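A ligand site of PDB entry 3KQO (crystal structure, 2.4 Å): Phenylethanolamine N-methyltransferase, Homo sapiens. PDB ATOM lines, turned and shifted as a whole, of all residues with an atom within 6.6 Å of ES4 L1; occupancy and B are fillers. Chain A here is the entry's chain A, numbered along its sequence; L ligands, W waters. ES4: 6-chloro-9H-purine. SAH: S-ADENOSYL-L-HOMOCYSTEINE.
Asn 39 touches ES4 L1. OH of Tyr 40 touches C08 of ES4 L1, 3.3 Å away. Val 53 touches ES4 L1 (CG2 to CL01, 3.7 Å). Phe 182 touches ES4 L1 (CE2 to C10, 3.4 Å). OE1 of Glu 219 touches C04 of ES4 L1, 3.3 Å away. OD2 of Asp 267 touches C04 of ES4 L1 (3.4 Å). CG1 of Val 269 touches N03 of ES4 L1 (3.8 Å). CG2 of Val 272 touches CL01 of ES4 L1, at 3.97 Å. Hydrophobic or aromatic side chains within 4 Å of ES4 L1: Tyr 35, Val 53, Phe 182, Val 269 and Val 272.
A nitrogen (N07) of ES4 L1 sits at hydrogen-bond distance from the side-chain hydroxyl of Tyr 35, 3.0 Å away. The side-chain amino group (NZ) of Lys 57 lies within hydrogen-bond range of a nitrogen (N09) of ES4 L1. NH1 of Arg 44 lies within hydrogen-bond range of N03 of ES4 L1, at 3.4 Å. The side-chain hydroxyl (OH) of Tyr 35 lies within hydrogen-bond range of an oxygen (OXT) of SAH L2 (2.5 Å). OH of Tyr 40 sits at hydrogen-bond distance from OXT of SAH L2 (2.6 Å). OH of Tyr 85 lies within hydrogen-bond range of O of SAH L2. The backbone carbonyl oxygen (O) of Ala 181 lies within hydrogen-bond range of a nitrogen (N) of SAH L2, at 3.0 Å.
NZ of Lys 57 is in hydrogen-bond range of OH of Tyr 40 (3.3 Å). OH of Tyr 85 lies within hydrogen-bond range of NZ of Lys 57. The side-chain hydroxyl (OH) of Tyr 85 lies close to the side-chain hydroxyl (OH) of Tyr 40 (3.0 Å). The side-chain amide oxygen of Asn 39 is in hydrogen-bond range of the guanidinium group of Arg 44 (2.9 Å). OD2 of Asp 267 is in salt-bridge range of NH1 of Arg 44 (2.8 Å). The side-chain carboxylate (OD1) of Asp 267 sits close to the backbone NH (N) of Val 269 (3.2 Å).
Water W3 bridges N05 of ES4 L1 (2.6 Å) and OE2 of Glu 219 (2.6 Å). Water W1 lies within hydrogen-bond range of N07 of ES4 L1 (2.9 Å), OH of Tyr 35 (3.5 Å) and SD of SAH L2 (3.7 Å). Water W2 lies within hydrogen-bond range of OD2 of Asp 267 (2.6 Å), ND2 of Asn 39 (2.9 Å) and N05 of ES4 L1 (3.4 Å).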
ATOM      1  N   TYR A  35      30.320  29.193 -13.422  1.00  0.00           N
ATOM      2  CA  TYR A  35      29.786  27.845 -13.472  1.00  0.00           C
ATOM      3  C   TYR A  35      30.725  26.836 -12.807  1.00  0.00           C
ATOM      4  O   TYR A  35      30.295  26.012 -12.006  1.00  0.00           O
ATOM      5  CB  TYR A  35      29.485  27.447 -14.914  1.00  0.00           C
ATOM      6  CG  TYR A  35      29.031  26.010 -15.103  1.00  0.00           C
ATOM      7  CD1 TYR A  35      27.722  25.635 -14.824  1.00  0.00           C
ATOM      8  CD2 TYR A  35      29.894  25.040 -15.578  1.00  0.00           C
ATOM      9  CE1 TYR A  35      27.291  24.327 -15.009  1.00  0.00           C
ATOM     10  CE2 TYR A  35      29.483  23.729 -15.773  1.00  0.00           C
ATOM     11  CZ  TYR A  35      28.182  23.381 -15.476  1.00  0.00           C
ATOM     12  OH  TYR A  35      27.772  22.080 -15.671  1.00  0.00           O
ATOM     13  N   ASN A  39      29.847  24.514  -9.399  1.00  0.00           N
ATOM     14  CA  ASN A  39      29.662  23.075  -9.454  1.00  0.00           C
ATOM     15  C   ASN A  39      30.914  22.231  -9.215  1.00  0.00           C
ATOM     16  O   ASN A  39      30.813  21.057  -8.871  1.00  0.00           O
ATOM     17  CB  ASN A  39      28.996  22.660 -10.769  1.00  0.00           C
ATOM     18  CG  ASN A  39      27.506  22.929 -10.764  1.00  0.00           C
ATOM     19  OD1 ASN A  39      26.751  22.276 -10.050  1.00  0.00           O
ATOM     20  ND2 ASN A  39      27.071  23.888 -11.571  1.00  0.00           N
ATOM     21  N   TYR A  40      32.085  22.825  -9.393  1.00  0.00           N
ATOM     22  CA  TYR A  40      33.302  22.028  -9.358  1.00  0.00           C
ATOM     23  C   TYR A  40      34.336  22.498  -8.361  1.00  0.00           C
ATOM     24  O   TYR A  40      35.416  21.913  -8.249  1.00  0.00           O
ATOM     25  CB  TYR A  40      33.865  21.885 -10.767  1.00  0.00           C
ATOM     26  CG  TYR A  40      32.877  21.162 -11.652  1.00  0.00           C
ATOM     27  CD1 TYR A  40      32.039  21.850 -12.517  1.00  0.00           C
ATOM     28  CD2 TYR A  40      32.745  19.786 -11.573  1.00  0.00           C
ATOM     29  CE1 TYR A  40      31.125  21.181 -13.302  1.00  0.00           C
ATOM     30  CE2 TYR A  40      31.847  19.112 -12.347  1.00  0.00           C
ATOM     31  CZ  TYR A  40      31.033  19.804 -13.209  1.00  0.00           C
ATOM     32  OH  TYR A  40      30.133  19.121 -13.984  1.00  0.00           O
ATOM     33  N   ARG A  44      30.431  21.152  -3.652  1.00  0.00           N
ATOM     34  CA  ARG A  44      30.163  20.128  -4.666  1.00  0.00           C
ATOM     35  C   ARG A  44      31.462  19.600  -5.239  1.00  0.00           C
ATOM     36  O   ARG A  44      31.501  18.512  -5.816  1.00  0.00           O
ATOM     37  CB  ARG A  44      29.277  20.667  -5.784  1.00  0.00           C
ATOM     38  CG  ARG A  44      27.888  21.071  -5.298  1.00  0.00           C
ATOM     39  CD  ARG A  44      26.984  21.481  -6.428  1.00  0.00           C
ATOM     40  NE  ARG A  44      25.627  21.682  -5.934  1.00  0.00           N
ATOM     41  CZ  ARG A  44      24.577  21.956  -6.706  1.00  0.00           C
ATOM     42  NH1 ARG A  44      24.735  22.064  -8.013  1.00  0.00           N
ATOM     43  NH2 ARG A  44      23.369  22.109  -6.160  1.00  0.00           N
ATOM     44  N   VAL A  53      28.603  14.316  -4.634  1.00  0.00           N
ATOM     45  CA  VAL A  53      28.176  14.131  -6.015  1.00  0.00           C
ATOM     46  C   VAL A  53      29.347  13.975  -6.986  1.00  0.00           C
ATOM     47  O   VAL A  53      29.258  13.241  -7.972  1.00  0.00           O
ATOM     48  CB  VAL A  53      27.250  15.296  -6.500  1.00  0.00           C
ATOM     49  CG1 VAL A  53      28.049  16.577  -6.707  1.00  0.00           C
ATOM     50  CG2 VAL A  53      26.542  14.895  -7.784  1.00  0.00           C
ATOM     51  N   GLY A  54      30.451  14.636  -6.688  1.00  0.00           N
ATOM     52  CA  GLY A  54      31.653  14.502  -7.493  1.00  0.00           C
ATOM     53  C   GLY A  54      32.105  13.052  -7.574  1.00  0.00           C
ATOM     54  O   GLY A  54      32.202  12.479  -8.650  1.00  0.00           O
ATOM     55  N   LYS A  57      29.683  10.825  -9.508  1.00  0.00           N
ATOM     56  CA  LYS A  57      29.809  10.961 -10.957  1.00  0.00           C
ATOM     57  C   LYS A  57      31.006  10.204 -11.517  1.00  0.00           C
ATOM     58  O   LYS A  57      30.875   9.467 -12.496  1.00  0.00           O
ATOM     59  CB  LYS A  57      29.853  12.433 -11.360  1.00  0.00           C
ATOM     60  CG  LYS A  57      28.564  13.174 -11.057  1.00  0.00           C
ATOM     61  CD  LYS A  57      28.343  14.382 -11.958  1.00  0.00           C
ATOM     62  CE  LYS A  57      29.304  15.512 -11.644  1.00  0.00           C
ATOM     63  NZ  LYS A  57      28.769  16.820 -12.092  1.00  0.00           N
ATOM     64  N   TYR A  85      36.291  16.463 -16.631  1.00  0.00           N
ATOM     65  CA  TYR A  85      36.204  15.298 -15.734  1.00  0.00           C
ATOM     66  C   TYR A  85      35.442  14.156 -16.384  1.00  0.00           C
ATOM     67  O   TYR A  85      35.729  12.987 -16.115  1.00  0.00           O
ATOM     68  CB  TYR A  85      35.474  15.667 -14.437  1.00  0.00           C
ATOM     69  CG  TYR A  85      33.987  15.862 -14.636  1.00  0.00           C
ATOM     70  CD1 TYR A  85      33.090  14.811 -14.458  1.00  0.00           C
ATOM     71  CD2 TYR A  85      33.481  17.087 -15.053  1.00  0.00           C
ATOM     72  CE1 TYR A  85      31.730  14.993 -14.667  1.00  0.00           C
ATOM     73  CE2 TYR A  85      32.121  17.268 -15.262  1.00  0.00           C
ATOM     74  CZ  TYR A  85      31.250  16.220 -15.067  1.00  0.00           C
ATOM     75  OH  TYR A  85      29.914  16.406 -15.272  1.00  0.00           O
ATOM     76  N   ALA A 181      27.051  15.252 -20.471  1.00  0.00           N
ATOM     77  CA  ALA A 181      26.798  15.499 -19.069  1.00  0.00           C
ATOM     78  C   ALA A 181      26.151  16.851 -18.891  1.00  0.00           C
ATOM     79  O   ALA A 181      26.735  17.867 -19.246  1.00  0.00           O
ATOM     80  CB  ALA A 181      28.107  15.428 -18.276  1.00  0.00           C
ATOM     81  N   PHE A 182      24.936  16.829 -18.339  1.00  0.00           N
ATOM     82  CA  PHE A 182      24.240  18.055 -17.942  1.00  0.00           C
ATOM     83  C   PHE A 182      23.994  19.007 -19.104  1.00  0.00           C
ATOM     84  O   PHE A 182      23.906  20.223 -18.910  1.00  0.00           O
ATOM     85  CB  PHE A 182      25.000  18.748 -16.826  1.00  0.00           C
ATOM     86  CG  PHE A 182      25.165  17.898 -15.609  1.00  0.00           C
ATOM     87  CD1 PHE A 182      26.294  17.121 -15.453  1.00  0.00           C
ATOM     88  CD2 PHE A 182      24.185  17.850 -14.643  1.00  0.00           C
ATOM     89  CE1 PHE A 182      26.440  16.320 -14.334  1.00  0.00           C
ATOM     90  CE2 PHE A 182      24.325  17.061 -13.528  1.00  0.00           C
ATOM     91  CZ  PHE A 182      25.456  16.294 -13.370  1.00  0.00           C
ATOM     92  N   GLU A 185      19.032  18.452 -20.863  1.00  0.00           N
ATOM     93  CA  GLU A 185      17.994  19.021 -20.015  1.00  0.00           C
ATOM     94  C   GLU A 185      18.246  20.507 -19.745  1.00  0.00           C
ATOM     95  O   GLU A 185      17.324  21.275 -19.494  1.00  0.00           O
ATOM     96  CB  GLU A 185      17.856  18.248 -18.702  1.00  0.00           C
ATOM     97  CG  GLU A 185      18.956  18.514 -17.673  1.00  0.00           C
ATOM     98  CD  GLU A 185      20.246  17.773 -17.976  1.00  0.00           C
ATOM     99  OE1 GLU A 185      20.298  17.035 -18.988  1.00  0.00           O
ATOM    100  OE2 GLU A 185      21.209  17.929 -17.198  1.00  0.00           O
ATOM    101  N   ALA A 216      20.916  16.476 -14.690  1.00  0.00           N
ATOM    102  CA  ALA A 216      20.199  16.943 -13.517  1.00  0.00           C
ATOM    103  C   ALA A 216      18.769  16.399 -13.466  1.00  0.00           C
ATOM    104  O   ALA A 216      18.115  16.271 -14.505  1.00  0.00           O
ATOM    105  CB  ALA A 216      20.193  18.444 -13.483  1.00  0.00           C
ATOM    106  N   GLU A 219      15.366  19.638 -12.037  1.00  0.00           N
ATOM    107  CA  GLU A 219      15.905  20.982 -11.960  1.00  0.00           C
ATOM    108  C   GLU A 219      15.166  21.884 -12.949  1.00  0.00           C
ATOM    109  O   GLU A 219      14.787  21.449 -14.034  1.00  0.00           O
ATOM    110  CB  GLU A 219      17.404  20.962 -12.271  1.00  0.00           C
ATOM    111  CG  GLU A 219      18.009  22.308 -12.584  1.00  0.00           C
ATOM    112  CD  GLU A 219      19.531  22.265 -12.626  1.00  0.00           C
ATOM    113  OE1 GLU A 219      20.127  21.521 -11.817  1.00  0.00           O
ATOM    114  OE2 GLU A 219      20.130  22.967 -13.457  1.00  0.00           O
ATOM    115  N   TYR A 222      19.377  27.235 -13.131  1.00  0.00           N
ATOM    116  CA  TYR A 222      20.659  27.373 -12.463  1.00  0.00           C
ATOM    117  C   TYR A 222      21.333  28.631 -12.973  1.00  0.00           C
ATOM    118  O   TYR A 222      21.004  29.152 -14.038  1.00  0.00           O
ATOM    119  CB  TYR A 222      21.541  26.149 -12.710  1.00  0.00           C
ATOM    120  CG  TYR A 222      22.143  26.076 -14.091  1.00  0.00           C
ATOM    121  CD1 TYR A 222      23.458  26.462 -14.318  1.00  0.00           C
ATOM    122  CD2 TYR A 222      21.388  25.635 -15.177  1.00  0.00           C
ATOM    123  CE1 TYR A 222      24.018  26.390 -15.582  1.00  0.00           C
ATOM    124  CE2 TYR A 222      21.939  25.556 -16.448  1.00  0.00           C
ATOM    125  CZ  TYR A 222      23.259  25.937 -16.647  1.00  0.00           C
ATOM    126  OH  TYR A 222      23.820  25.882 -17.886  1.00  0.00           O
ATOM    127  N   MET A 258      20.446  14.411  -4.254  1.00  0.00           N
ATOM    128  CA  MET A 258      21.292  15.526  -3.813  1.00  0.00           C
ATOM    129  C   MET A 258      21.083  15.846  -2.332  1.00  0.00           C
ATOM    130  O   MET A 258      19.989  16.233  -1.924  1.00  0.00           O
ATOM    131  CB  MET A 258      21.044  16.755  -4.684  1.00  0.00           C
ATOM    132  CG  MET A 258      22.102  17.846  -4.583  1.00  0.00           C
ATOM    133  SD  MET A 258      23.655  17.449  -5.418  1.00  0.00           S
ATOM    134  CE  MET A 258      23.076  16.740  -6.955  1.00  0.00           C
ATOM    135  N   VAL A 266      22.834  27.910  -6.045  1.00  0.00           N
ATOM    136  CA  VAL A 266      23.246  28.073  -7.444  1.00  0.00           C
ATOM    137  C   VAL A 266      22.227  27.494  -8.421  1.00  0.00           C
ATOM    138  O   VAL A 266      22.225  27.831  -9.592  1.00  0.00           O
ATOM    139  CB  VAL A 266      24.627  27.437  -7.745  1.00  0.00           C
ATOM    140  CG1 VAL A 266      25.708  28.046  -6.846  1.00  0.00           C
ATOM    141  CG2 VAL A 266      24.563  25.915  -7.609  1.00  0.00           C
ATOM    142  N   ASP A 267      21.373  26.604  -7.922  1.00  0.00           N
ATOM    143  CA  ASP A 267      20.335  25.985  -8.742  1.00  0.00           C
ATOM    144  C   ASP A 267      19.288  25.334  -7.852  1.00  0.00           C
ATOM    145  O   ASP A 267      19.304  25.504  -6.642  1.00  0.00           O
ATOM    146  CB  ASP A 267      20.945  24.954  -9.716  1.00  0.00           C
ATOM    147  CG  ASP A 267      21.751  23.884  -9.009  1.00  0.00           C
ATOM    148  OD1 ASP A 267      21.278  23.344  -7.981  1.00  0.00           O
ATOM    149  OD2 ASP A 267      22.863  23.565  -9.489  1.00  0.00           O
ATOM    150  N   VAL A 269      18.508  21.819  -8.319  1.00  0.00           N
ATOM    151  CA  VAL A 269      18.634  20.412  -8.670  1.00  0.00           C
ATOM    152  C   VAL A 269      18.229  19.557  -7.479  1.00  0.00           C
ATOM    153  O   VAL A 269      18.483  19.915  -6.335  1.00  0.00           O
ATOM    154  CB  VAL A 269      20.082  20.071  -9.104  1.00  0.00           C
ATOM    155  CG1 VAL A 269      21.042  20.294  -7.941  1.00  0.00           C
ATOM    156  CG2 VAL A 269      20.184  18.619  -9.605  1.00  0.00           C
ATOM    157  N   GLY A 271      18.466  15.856  -7.800  1.00  0.00           N
ATOM    158  CA  GLY A 271      19.244  14.633  -7.912  1.00  0.00           C
ATOM    159  C   GLY A 271      20.019  14.616  -9.211  1.00  0.00           C
ATOM    160  O   GLY A 271      19.924  15.547 -10.017  1.00  0.00           O
ATOM    161  N   VAL A 272      20.811  13.579  -9.408  1.00  0.00           N
ATOM    162  CA  VAL A 272      21.571  13.442 -10.646  1.00  0.00           C
ATOM    163  C   VAL A 272      21.337  12.054 -11.193  1.00  0.00           C
ATOM    164  O   VAL A 272      21.324  11.082 -10.449  1.00  0.00           O
ATOM    165  CB  VAL A 272      23.094  13.637 -10.419  1.00  0.00           C
ATOM    166  CG1 VAL A 272      23.862  13.263 -11.665  1.00  0.00           C
ATOM    167  CG2 VAL A 272      23.384  15.072  -9.990  1.00  0.00           C
HETATM  168  C10 ES4 L   1      25.704  19.641 -11.863  1.00  0.00           C
HETATM  169 CL01 ES4 L   1      25.978  18.061  -9.624  1.00  0.00          CL
HETATM  170  C02 ES4 L   1      25.136  19.240 -10.669  1.00  0.00           C
HETATM  171  N03 ES4 L   1      23.929  19.738 -10.301  1.00  0.00           N
HETATM  172  C04 ES4 L   1      23.273  20.637 -11.101  1.00  0.00           C
HETATM  173  N05 ES4 L   1      23.849  21.036 -12.290  1.00  0.00           N
HETATM  174  C06 ES4 L   1      25.048  20.540 -12.664  1.00  0.00           C
HETATM  175  N07 ES4 L   1      25.819  20.761 -13.758  1.00  0.00           N
HETATM  176  C08 ES4 L   1      26.943  19.990 -13.630  1.00  0.00           C
HETATM  177  N09 ES4 L   1      26.863  19.298 -12.458  1.00  0.00           N
HETATM  178  N   SAH L   2      29.450  18.951 -19.687  1.00  0.00           N
HETATM  179  CA  SAH L   2      29.332  20.038 -18.717  1.00  0.00           C
HETATM  180  CB  SAH L   2      27.921  20.635 -18.812  1.00  0.00           C
HETATM  181  CG  SAH L   2      28.025  22.146 -18.993  1.00  0.00           C
HETATM  182  SD  SAH L   2      26.404  22.895 -18.637  1.00  0.00           S
HETATM  183  C   SAH L   2      29.494  19.419 -17.319  1.00  0.00           C
HETATM  184  O   SAH L   2      29.392  18.246 -17.194  1.00  0.00           O
HETATM  185  OXT SAH L   2      29.354  20.241 -16.196  1.00  0.00           O
HETATM  186  C5' SAH L   2      25.366  22.857 -20.117  1.00  0.00           C
HETATM  187  C4' SAH L   2      26.242  23.058 -21.358  1.00  0.00           C
HETATM  188  O4' SAH L   2      25.402  22.981 -22.559  1.00  0.00           O
HETATM  189  C3' SAH L   2      26.921  24.440 -21.379  1.00  0.00           C
HETATM  190  O3' SAH L   2      28.299  24.293 -21.640  1.00  0.00           O
HETATM  191  C2' SAH L   2      26.237  25.098 -22.539  1.00  0.00           C
HETATM  192  O2' SAH L   2      26.917  26.163 -23.143  1.00  0.00           O
HETATM  193  C1' SAH L   2      25.973  23.941 -23.491  1.00  0.00           C
HETATM  194  N9  SAH L   2      24.964  24.366 -24.440  1.00  0.00           N
HETATM  195  C8  SAH L   2      24.116  25.578 -24.303  1.00  0.00           C
HETATM  196  N7  SAH L   2      23.210  25.610 -25.451  1.00  0.00           N
HETATM  197  C5  SAH L   2      23.494  24.428 -26.285  1.00  0.00           C
HETATM  198  C6  SAH L   2      22.875  23.948 -27.569  1.00  0.00           C
HETATM  199  N6  SAH L   2      21.796  24.720 -28.187  1.00  0.00           N
HETATM  200  N1  SAH L   2      23.366  22.722 -28.178  1.00  0.00           N
HETATM  201  C2  SAH L   2      24.470  21.930 -27.532  1.00  0.00           C
HETATM  202  N3  SAH L   2      25.079  22.416 -26.267  1.00  0.00           N
HETATM  203  C4  SAH L   2      24.586  23.661 -25.647  1.00  0.00           C
HETATM  204  O   HOH W   1      24.297  22.189 -15.711  1.00  0.00           O
HETATM  205  O   HOH W   2      24.161  24.358 -11.550  1.00  0.00           O
HETATM  206  O   HOH W   3      22.713  22.810 -13.831  1.00  0.00           O
